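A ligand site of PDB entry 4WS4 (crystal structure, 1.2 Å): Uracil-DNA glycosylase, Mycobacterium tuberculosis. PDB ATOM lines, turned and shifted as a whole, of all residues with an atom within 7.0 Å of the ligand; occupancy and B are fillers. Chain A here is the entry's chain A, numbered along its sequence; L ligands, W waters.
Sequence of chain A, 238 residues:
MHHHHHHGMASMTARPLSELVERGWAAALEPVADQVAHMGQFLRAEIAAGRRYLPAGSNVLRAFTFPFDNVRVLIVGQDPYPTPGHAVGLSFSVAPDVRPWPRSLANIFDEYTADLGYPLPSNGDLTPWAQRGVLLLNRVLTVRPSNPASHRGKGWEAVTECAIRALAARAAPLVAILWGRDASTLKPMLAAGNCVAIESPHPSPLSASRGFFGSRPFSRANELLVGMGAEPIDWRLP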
ATOM      1  N   VAL A  76     -17.437 -27.352 -17.880  1.00  0.00           N
ATOM      2  CA  VAL A  76     -17.026 -26.055 -17.363  1.00  0.00           C
ATOM      3  C   VAL A  76     -18.225 -25.124 -17.286  1.00  0.00           C
ATOM      4  O   VAL A  76     -18.890 -24.867 -18.303  1.00  0.00           O
ATOM      5  CB  VAL A  76     -15.915 -25.376 -18.171  1.00  0.00           C
ATOM      6  CG1 VAL A  76     -15.387 -24.161 -17.436  1.00  0.00           C
ATOM      7  CG2 VAL A  76     -14.791 -26.355 -18.472  1.00  0.00           C
ATOM      8  N   GLY A  77     -18.505 -24.608 -16.079  1.00  0.00           N
ATOM      9  CA  GLY A  77     -19.427 -23.495 -15.896  1.00  0.00           C
ATOM     10  C   GLY A  77     -18.736 -22.170 -15.666  1.00  0.00           C
ATOM     11  O   GLY A  77     -17.551 -21.980 -16.002  1.00  0.00           O
ATOM     12  N   GLN A  78     -19.480 -21.239 -15.089  1.00  0.00           N
ATOM     13  CA  GLN A  78     -19.033 -19.886 -14.890  1.00  0.00           C
ATOM     14  C   GLN A  78     -18.227 -19.703 -13.616  1.00  0.00           C
ATOM     15  O   GLN A  78     -17.032 -19.324 -13.634  1.00  0.00           O
ATOM     16  CB  GLN A  78     -20.229 -18.923 -14.930  1.00  0.00           C
ATOM     17  CG  GLN A  78     -19.842 -17.492 -14.667  1.00  0.00           C
ATOM     18  CD  GLN A  78     -21.023 -16.562 -14.706  1.00  0.00           C
ATOM     19  OE1 GLN A  78     -21.605 -16.257 -13.639  1.00  0.00           O
ATOM     20  NE2 GLN A  78     -21.397 -16.166 -15.867  1.00  0.00           N
ATOM     21  N   ASP A  79     -18.916 -19.868 -12.498  1.00  0.00           N
ATOM     22  CA  ASP A  79     -18.370 -19.643 -11.158  1.00  0.00           C
ATOM     23  C   ASP A  79     -19.286 -20.343 -10.159  1.00  0.00           C
ATOM     24  O   ASP A  79     -20.348 -20.818 -10.546  1.00  0.00           O
ATOM     25  CB  ASP A  79     -18.152 -18.146 -10.879  1.00  0.00           C
ATOM     26  CG  ASP A  79     -19.430 -17.301 -10.699  1.00  0.00           C
ATOM     27  OD1 ASP A  79     -20.468 -17.640 -11.323  1.00  0.00           O
ATOM     28  OD2 ASP A  79     -19.382 -16.281  -9.985  1.00  0.00           O
ATOM     29  N   PRO A  80     -18.867 -20.451  -8.884  1.00  0.00           N
ATOM     30  CA  PRO A  80     -19.663 -21.275  -7.974  1.00  0.00           C
ATOM     31  C   PRO A  80     -21.030 -20.685  -7.619  1.00  0.00           C
ATOM     32  O   PRO A  80     -21.262 -19.472  -7.771  1.00  0.00           O
ATOM     33  CB  PRO A  80     -18.785 -21.330  -6.723  1.00  0.00           C
ATOM     34  CG  PRO A  80     -17.377 -21.107  -7.230  1.00  0.00           C
ATOM     35  CD  PRO A  80     -17.567 -20.091  -8.313  1.00  0.00           C
ATOM     36  N   TYR A  81     -21.889 -21.535  -7.078  1.00  0.00           N
ATOM     37  CA  TYR A  81     -23.197 -21.049  -6.609  1.00  0.00           C
ATOM     38  C   TYR A  81     -22.994 -19.898  -5.631  1.00  0.00           C
ATOM     39  O   TYR A  81     -22.137 -19.981  -4.740  1.00  0.00           O
ATOM     40  CB  TYR A  81     -23.952 -22.134  -5.883  1.00  0.00           C
ATOM     41  CG  TYR A  81     -24.509 -23.235  -6.809  1.00  0.00           C
ATOM     42  CD1 TYR A  81     -25.429 -22.943  -7.800  1.00  0.00           C
ATOM     43  CD2 TYR A  81     -24.090 -24.540  -6.676  1.00  0.00           C
ATOM     44  CE1 TYR A  81     -25.914 -23.921  -8.620  1.00  0.00           C
ATOM     45  CE2 TYR A  81     -24.563 -25.537  -7.497  1.00  0.00           C
ATOM     46  CZ  TYR A  81     -25.480 -25.237  -8.494  1.00  0.00           C
ATOM     47  OH  TYR A  81     -25.998 -26.187  -9.352  1.00  0.00           O
ATOM     48  N   PRO A  82     -23.832 -18.864  -5.683  1.00  0.00           N
ATOM     49  CA  PRO A  82     -23.691 -17.717  -4.788  1.00  0.00           C
ATOM     50  C   PRO A  82     -24.363 -17.854  -3.421  1.00  0.00           C
ATOM     51  O   PRO A  82     -24.160 -17.006  -2.583  1.00  0.00           O
ATOM     52  CB  PRO A  82     -24.308 -16.587  -5.599  1.00  0.00           C
ATOM     53  CG  PRO A  82     -25.452 -17.276  -6.333  1.00  0.00           C
ATOM     54  CD  PRO A  82     -24.783 -18.566  -6.796  1.00  0.00           C
ATOM     55  N   ALA A  87     -22.410 -24.238  -2.918  1.00  0.00           N
ATOM     56  CA  ALA A  87     -21.186 -24.637  -3.632  1.00  0.00           C
ATOM     57  C   ALA A  87     -20.349 -25.576  -2.780  1.00  0.00           C
ATOM     58  O   ALA A  87     -20.129 -25.331  -1.591  1.00  0.00           O
ATOM     59  CB  ALA A  87     -20.359 -23.431  -4.018  1.00  0.00           C
ATOM     60  N   LEU A  90     -17.173 -28.713  -6.644  1.00  0.00           N
ATOM     61  CA  LEU A  90     -17.389 -29.453  -7.888  1.00  0.00           C
ATOM     62  C   LEU A  90     -18.503 -28.655  -8.591  1.00  0.00           C
ATOM     63  O   LEU A  90     -19.567 -28.464  -8.000  1.00  0.00           O
ATOM     64  CB  LEU A  90     -17.862 -30.893  -7.623  1.00  0.00           C
ATOM     65  CG  LEU A  90     -16.800 -31.742  -6.915  1.00  0.00           C
ATOM     66  CD1 LEU A  90     -17.391 -33.118  -6.604  1.00  0.00           C
ATOM     67  CD2 LEU A  90     -15.504 -31.872  -7.707  1.00  0.00           C
ATOM     68  N   SER A  91     -18.254 -28.201  -9.806  1.00  0.00           N
ATOM     69  CA  SER A  91     -19.228 -27.313 -10.438  1.00  0.00           C
ATOM     70  C   SER A  91     -20.600 -27.975 -10.506  1.00  0.00           C
ATOM     71  O   SER A  91     -20.753 -29.164 -10.758  1.00  0.00           O
ATOM     72  CB  SER A  91     -18.751 -26.815 -11.767  1.00  0.00           C
ATOM     73  OG  SER A  91     -18.627 -27.862 -12.696  1.00  0.00           O
ATOM     74  N   PHE A  92     -21.589 -27.151 -10.163  1.00  0.00           N
ATOM     75  CA  PHE A  92     -23.010 -27.463 -10.204  1.00  0.00           C
ATOM     76  C   PHE A  92     -23.509 -28.419  -9.131  1.00  0.00           C
ATOM     77  O   PHE A  92     -24.730 -28.527  -8.943  1.00  0.00           O
ATOM     78  CB  PHE A  92     -23.458 -27.919 -11.613  1.00  0.00           C
ATOM     79  CG  PHE A  92     -23.229 -26.874 -12.670  1.00  0.00           C
ATOM     80  CD1 PHE A  92     -24.061 -25.783 -12.786  1.00  0.00           C
ATOM     81  CD2 PHE A  92     -22.126 -26.937 -13.479  1.00  0.00           C
ATOM     82  CE1 PHE A  92     -23.832 -24.809 -13.739  1.00  0.00           C
ATOM     83  CE2 PHE A  92     -21.869 -25.978 -14.434  1.00  0.00           C
ATOM     84  CZ  PHE A  92     -22.722 -24.903 -14.568  1.00  0.00           C
ATOM     85  N   SER A  93     -22.621 -29.095  -8.431  1.00  0.00           N
ATOM     86  CA  SER A  93     -23.011 -30.071  -7.441  1.00  0.00           C
ATOM     87  C   SER A  93     -23.469 -29.420  -6.147  1.00  0.00           C
ATOM     88  O   SER A  93     -23.001 -28.329  -5.784  1.00  0.00           O
ATOM     89  CB  SER A  93     -21.803 -30.972  -7.163  1.00  0.00           C
ATOM     90  OG  SER A  93     -22.180 -32.155  -6.500  1.00  0.00           O
ATOM     91  N   PRO A 102     -30.722 -25.686  -6.619  1.00  0.00           N
ATOM     92  CA  PRO A 102     -30.556 -24.424  -7.330  1.00  0.00           C
ATOM     93  C   PRO A 102     -31.095 -24.579  -8.753  1.00  0.00           C
ATOM     94  O   PRO A 102     -31.103 -25.674  -9.325  1.00  0.00           O
ATOM     95  CB  PRO A 102     -29.044 -24.186  -7.313  1.00  0.00           C
ATOM     96  CG  PRO A 102     -28.450 -25.286  -6.586  1.00  0.00           C
ATOM     97  CD  PRO A 102     -29.449 -26.257  -6.156  1.00  0.00           C
ATOM     98  N   SER A 104     -30.034 -23.702 -11.776  1.00  0.00           N
ATOM     99  CA  SER A 104     -29.165 -24.237 -12.840  1.00  0.00           C
ATOM    100  C   SER A 104     -29.143 -25.768 -12.788  1.00  0.00           C
ATOM    101  O   SER A 104     -29.177 -26.417 -13.824  1.00  0.00           O
ATOM    102  CB  SER A 104     -27.717 -23.718 -12.770  1.00  0.00           C
ATOM    103  OG  SER A 104     -27.543 -22.426 -13.254  1.00  0.00           O
ATOM    104  N   LEU A 105     -29.101 -26.316 -11.564  1.00  0.00           N
ATOM    105  CA  LEU A 105     -29.055 -27.759 -11.395  1.00  0.00           C
ATOM    106  C   LEU A 105     -30.386 -28.391 -11.813  1.00  0.00           C
ATOM    107  O   LEU A 105     -30.401 -29.434 -12.465  1.00  0.00           O
ATOM    108  CB  LEU A 105     -28.678 -28.140  -9.958  1.00  0.00           C
ATOM    109  CG  LEU A 105     -28.441 -29.617  -9.745  1.00  0.00           C
ATOM    110  CD1 LEU A 105     -27.346 -30.143 -10.665  1.00  0.00           C
ATOM    111  CD2 LEU A 105     -28.059 -29.824  -8.303  1.00  0.00           C
ATOM    112  N   LEU A 136     -15.534 -31.503 -12.999  1.00  0.00           N
ATOM    113  CA  LEU A 136     -16.588 -30.510 -12.779  1.00  0.00           C
ATOM    114  C   LEU A 136     -15.967 -29.194 -12.407  1.00  0.00           C
ATOM    115  O   LEU A 136     -15.801 -28.841 -11.234  1.00  0.00           O
ATOM    116  CB  LEU A 136     -17.592 -31.015 -11.716  1.00  0.00           C
ATOM    117  CG  LEU A 136     -18.352 -32.293 -12.147  1.00  0.00           C
ATOM    118  CD1 LEU A 136     -19.118 -32.883 -10.988  1.00  0.00           C
ATOM    119  CD2 LEU A 136     -19.322 -31.969 -13.256  1.00  0.00           C
ATOM    120  N   LEU A 137     -15.567 -28.455 -13.440  1.00  0.00           N
ATOM    121  CA  LEU A 137     -14.833 -27.190 -13.282  1.00  0.00           C
ATOM    122  C   LEU A 137     -15.736 -25.976 -13.512  1.00  0.00           C
ATOM    123  O   LEU A 137     -16.795 -26.084 -14.108  1.00  0.00           O
ATOM    124  CB  LEU A 137     -13.690 -27.176 -14.304  1.00  0.00           C
ATOM    125  CG  LEU A 137     -12.486 -26.303 -14.005  1.00  0.00           C
ATOM    126  CD1 LEU A 137     -11.841 -26.586 -12.656  1.00  0.00           C
ATOM    127  CD2 LEU A 137     -11.479 -26.402 -15.145  1.00  0.00           C
ATOM    128  N   ASN A 138     -15.286 -24.842 -13.012  1.00  0.00           N
ATOM    129  CA  ASN A 138     -15.797 -23.527 -13.391  1.00  0.00           C
ATOM    130  C   ASN A 138     -14.655 -22.702 -13.943  1.00  0.00           C
ATOM    131  O   ASN A 138     -13.506 -22.903 -13.548  1.00  0.00           O
ATOM    132  CB  ASN A 138     -16.421 -22.836 -12.188  1.00  0.00           C
ATOM    133  CG  ASN A 138     -17.798 -23.351 -11.860  1.00  0.00           C
ATOM    134  OD1 ASN A 138     -18.642 -23.480 -12.741  1.00  0.00           O
ATOM    135  ND2 ASN A 138     -18.047 -23.620 -10.575  1.00  0.00           N
ATOM    136  N   ARG A 139     -14.967 -21.677 -14.750  1.00  0.00           N
ATOM    137  CA  ARG A 139     -13.900 -20.814 -15.264  1.00  0.00           C
ATOM    138  C   ARG A 139     -13.213 -20.054 -14.117  1.00  0.00           C
ATOM    139  O   ARG A 139     -12.002 -19.800 -14.149  1.00  0.00           O
ATOM    140  CB  ARG A 139     -14.506 -19.869 -16.282  1.00  0.00           C
ATOM    141  CG  ARG A 139     -13.470 -19.093 -17.100  1.00  0.00           C
ATOM    142  CD  ARG A 139     -12.726 -19.969 -18.110  1.00  0.00           C
ATOM    143  NE  ARG A 139     -11.932 -19.161 -19.026  1.00  0.00           N
ATOM    144  CZ  ARG A 139     -10.653 -18.837 -18.863  1.00  0.00           C
ATOM    145  NH1 ARG A 139      -9.929 -19.379 -17.906  1.00  0.00           N
ATOM    146  NH2 ARG A 139     -10.077 -18.014 -19.721  1.00  0.00           N
ATOM    147  N   VAL A 140     -14.013 -19.689 -13.113  1.00  0.00           N
ATOM    148  CA  VAL A 140     -13.562 -18.980 -11.920  1.00  0.00           C
ATOM    149  C   VAL A 140     -14.011 -19.791 -10.708  1.00  0.00           C
ATOM    150  O   VAL A 140     -15.120 -20.310 -10.697  1.00  0.00           O
ATOM    151  CB  VAL A 140     -14.156 -17.548 -11.940  1.00  0.00           C
ATOM    152  CG1 VAL A 140     -14.058 -16.840 -10.600  1.00  0.00           C
ATOM    153  CG2 VAL A 140     -13.526 -16.744 -13.059  1.00  0.00           C
ATOM    154  N   PRO A 148     -23.209 -13.309  -8.064  1.00  0.00           N
ATOM    155  CA  PRO A 148     -22.650 -14.040  -9.219  1.00  0.00           C
ATOM    156  C   PRO A 148     -21.632 -13.219 -10.003  1.00  0.00           C
ATOM    157  O   PRO A 148     -21.849 -12.010 -10.241  1.00  0.00           O
ATOM    158  CB  PRO A 148     -23.877 -14.365 -10.074  1.00  0.00           C
ATOM    159  CG  PRO A 148     -25.014 -14.389  -9.116  1.00  0.00           C
ATOM    160  CD  PRO A 148     -24.683 -13.379  -8.046  1.00  0.00           C
ATOM    161  N   TRP A 179     -20.340 -24.603 -20.811  1.00  0.00           N
ATOM    162  CA  TRP A 179     -21.666 -24.044 -20.525  1.00  0.00           C
ATOM    163  C   TRP A 179     -21.531 -22.549 -20.250  1.00  0.00           C
ATOM    164  O   TRP A 179     -21.078 -22.143 -19.160  1.00  0.00           O
ATOM    165  CB  TRP A 179     -22.350 -24.773 -19.358  1.00  0.00           C
ATOM    166  CG  TRP A 179     -22.872 -26.120 -19.724  1.00  0.00           C
ATOM    167  CD1 TRP A 179     -23.230 -26.548 -20.964  1.00  0.00           C
ATOM    168  CD2 TRP A 179     -23.203 -27.198 -18.853  1.00  0.00           C
ATOM    169  NE1 TRP A 179     -23.704 -27.827 -20.915  1.00  0.00           N
ATOM    170  CE2 TRP A 179     -23.686 -28.255 -19.616  1.00  0.00           C
ATOM    171  CE3 TRP A 179     -23.086 -27.367 -17.481  1.00  0.00           C
ATOM    172  CZ2 TRP A 179     -24.064 -29.471 -19.056  1.00  0.00           C
ATOM    173  CZ3 TRP A 179     -23.469 -28.562 -16.912  1.00  0.00           C
ATOM    174  CH2 TRP A 179     -23.935 -29.602 -17.695  1.00  0.00           C
ATOM    175  N   HIS A 202     -25.518 -21.488 -21.152  1.00  0.00           N
ATOM    176  CA  HIS A 202     -25.501 -21.924 -19.773  1.00  0.00           C
ATOM    177  C   HIS A 202     -26.884 -22.396 -19.316  1.00  0.00           C
ATOM    178  O   HIS A 202     -27.897 -21.878 -19.789  1.00  0.00           O
ATOM    179  CB  HIS A 202     -24.990 -20.738 -18.962  1.00  0.00           C
ATOM    180  CG  HIS A 202     -24.660 -21.038 -17.536  1.00  0.00           C
ATOM    181  ND1 HIS A 202     -25.621 -21.198 -16.574  1.00  0.00           N
ATOM    182  CD2 HIS A 202     -23.454 -21.130 -16.916  1.00  0.00           C
ATOM    183  CE1 HIS A 202     -25.028 -21.433 -15.412  1.00  0.00           C
ATOM    184  NE2 HIS A 202     -23.708 -21.355 -15.594  1.00  0.00           N
ATOM    185  N   PRO A 203     -26.942 -23.392 -18.425  1.00  0.00           N
ATOM    186  CA  PRO A 203     -28.225 -23.898 -17.948  1.00  0.00           C
ATOM    187  C   PRO A 203     -28.995 -22.967 -17.043  1.00  0.00           C
ATOM    188  O   PRO A 203     -30.136 -23.288 -16.674  1.00  0.00           O
ATOM    189  CB  PRO A 203     -27.870 -25.196 -17.232  1.00  0.00           C
ATOM    190  CG  PRO A 203     -26.429 -25.002 -16.812  1.00  0.00           C
ATOM    191  CD  PRO A 203     -25.814 -24.211 -17.942  1.00  0.00           C
ATOM    192  N   SER A 204     -28.424 -21.848 -16.610  1.00  0.00           N
ATOM    193  CA  SER A 204     -29.163 -20.896 -15.800  1.00  0.00           C
ATOM    194  C   SER A 204     -30.472 -20.535 -16.502  1.00  0.00           C
ATOM    195  O   SER A 204     -30.537 -20.397 -17.719  1.00  0.00           O
ATOM    196  CB  SER A 204     -28.341 -19.651 -15.683  1.00  0.00           C
ATOM    197  OG  SER A 204     -29.125 -18.545 -15.312  1.00  0.00           O
HETATM  198  O1  LIG L   1     -21.768 -21.757 -13.586  1.00  0.00           O
HETATM  199  C1  LIG L   1     -22.106 -22.208 -12.463  1.00  0.00           C
HETATM  200  N1  LIG L   1     -21.335 -23.169 -11.865  1.00  0.00           N
HETATM  201  C2  LIG L   1     -21.664 -23.638 -10.652  1.00  0.00           C
HETATM  202  O2  LIG L   1     -20.769 -24.426 -10.080  1.00  0.00           O
HETATM  203  N2  LIG L   1     -22.732 -23.308  -9.945  1.00  0.00           N
HETATM  204  C3  LIG L   1     -23.499 -22.372 -10.485  1.00  0.00           C
HETATM  205  C4  LIG L   1     -23.249 -21.840 -11.718  1.00  0.00           C
HETATM  206  N3  LIG L   1     -24.069 -20.779 -12.140  1.00  0.00           N
HETATM  207  O3  LIG L   1     -25.144 -20.489 -11.439  1.00  0.00           O
HETATM  208  O4  LIG L   1     -23.644 -19.864 -12.990  1.00  0.00           O
HETATM  209  O   HOH W   1     -20.735 -24.327  -7.326  1.00  0.00           O
HETATM  210  O   HOH W   2     -25.246 -18.029 -14.072  1.00  0.00           O
HETATM  211  O   HOH W   3     -25.117 -17.867 -10.187  1.00  0.00           O
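N1 of the ligand sits at hydrogen-bond distance from OD1 of Asn 138 (2.8 Å). An oxygen (O1) of the ligand is in hydrogen-bond range of the backbone NH (N) of Gln 78, at 2.8 Å. NE2 of His 202 lies within hydrogen-bond range of O1 of the ligand (2.8 Å). N1 of the ligand lies within hydrogen-bond range of O of Asp 79, 2.9 Å away. The backbone NH (N) of Phe 92 is in hydrogen-bond range of an oxygen (O2) of the ligand (2.8 Å).
The backbone NH (N) of Arg 139 is in hydrogen-bond range of the backbone carbonyl oxygen (O) of Gln 78 (3.3 Å). ND1 of His 202 sits at hydrogen-bond distance from N of Ser 204, 2.9 Å away. The backbone carbonyl oxygen (O) of Gly 77 sits at hydrogen-bond distance from the backbone NH (N) of Arg 139, 2.9 Å away. The side-chain amide oxygen (OE1) of Gln 78 sits close to the side-chain carboxylate (OD1) of Asp 79, at 2.9 Å. The backbone carbonyl oxygen of Gln 78 lies within hydrogen-bond range of the backbone NH of Val 140, 3.1 Å away. The backbone carbonyl oxygen (O) of Phe 92 is in hydrogen-bond range of the side-chain hydroxyl (OH) of Tyr 81 (2.7 Å). N of Gly 77 is in hydrogen-bond range of O of Leu 137 (3.0 Å). The backbone carbonyl oxygen (O) of Leu 137 sits at hydrogen-bond distance from the side-chain hydroxyl (OG) of Ser 91, 2.9 Å away.
The backbone NH (N) of Tyr 81 lies close to a nitrogen (N2) of the ligand (3.5 Å). Gly 77 touches the ligand (C to O1, 3.7 Å). C of Pro 80 touches N2 of the ligand, at 3.9 Å. Ser 91 touches the ligand. OG of Ser 104 touches O3 of the ligand, at 3.6 Å. Hydrophobic or aromatic side chains that line the ligand: Tyr 81, Phe 92 and His 202. The nearest printed residue that does not touch the ligand is Leu 90 (4.7 Å).
Water W1 lies within hydrogen-bond range of O2 of the ligand and N of Tyr 81.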
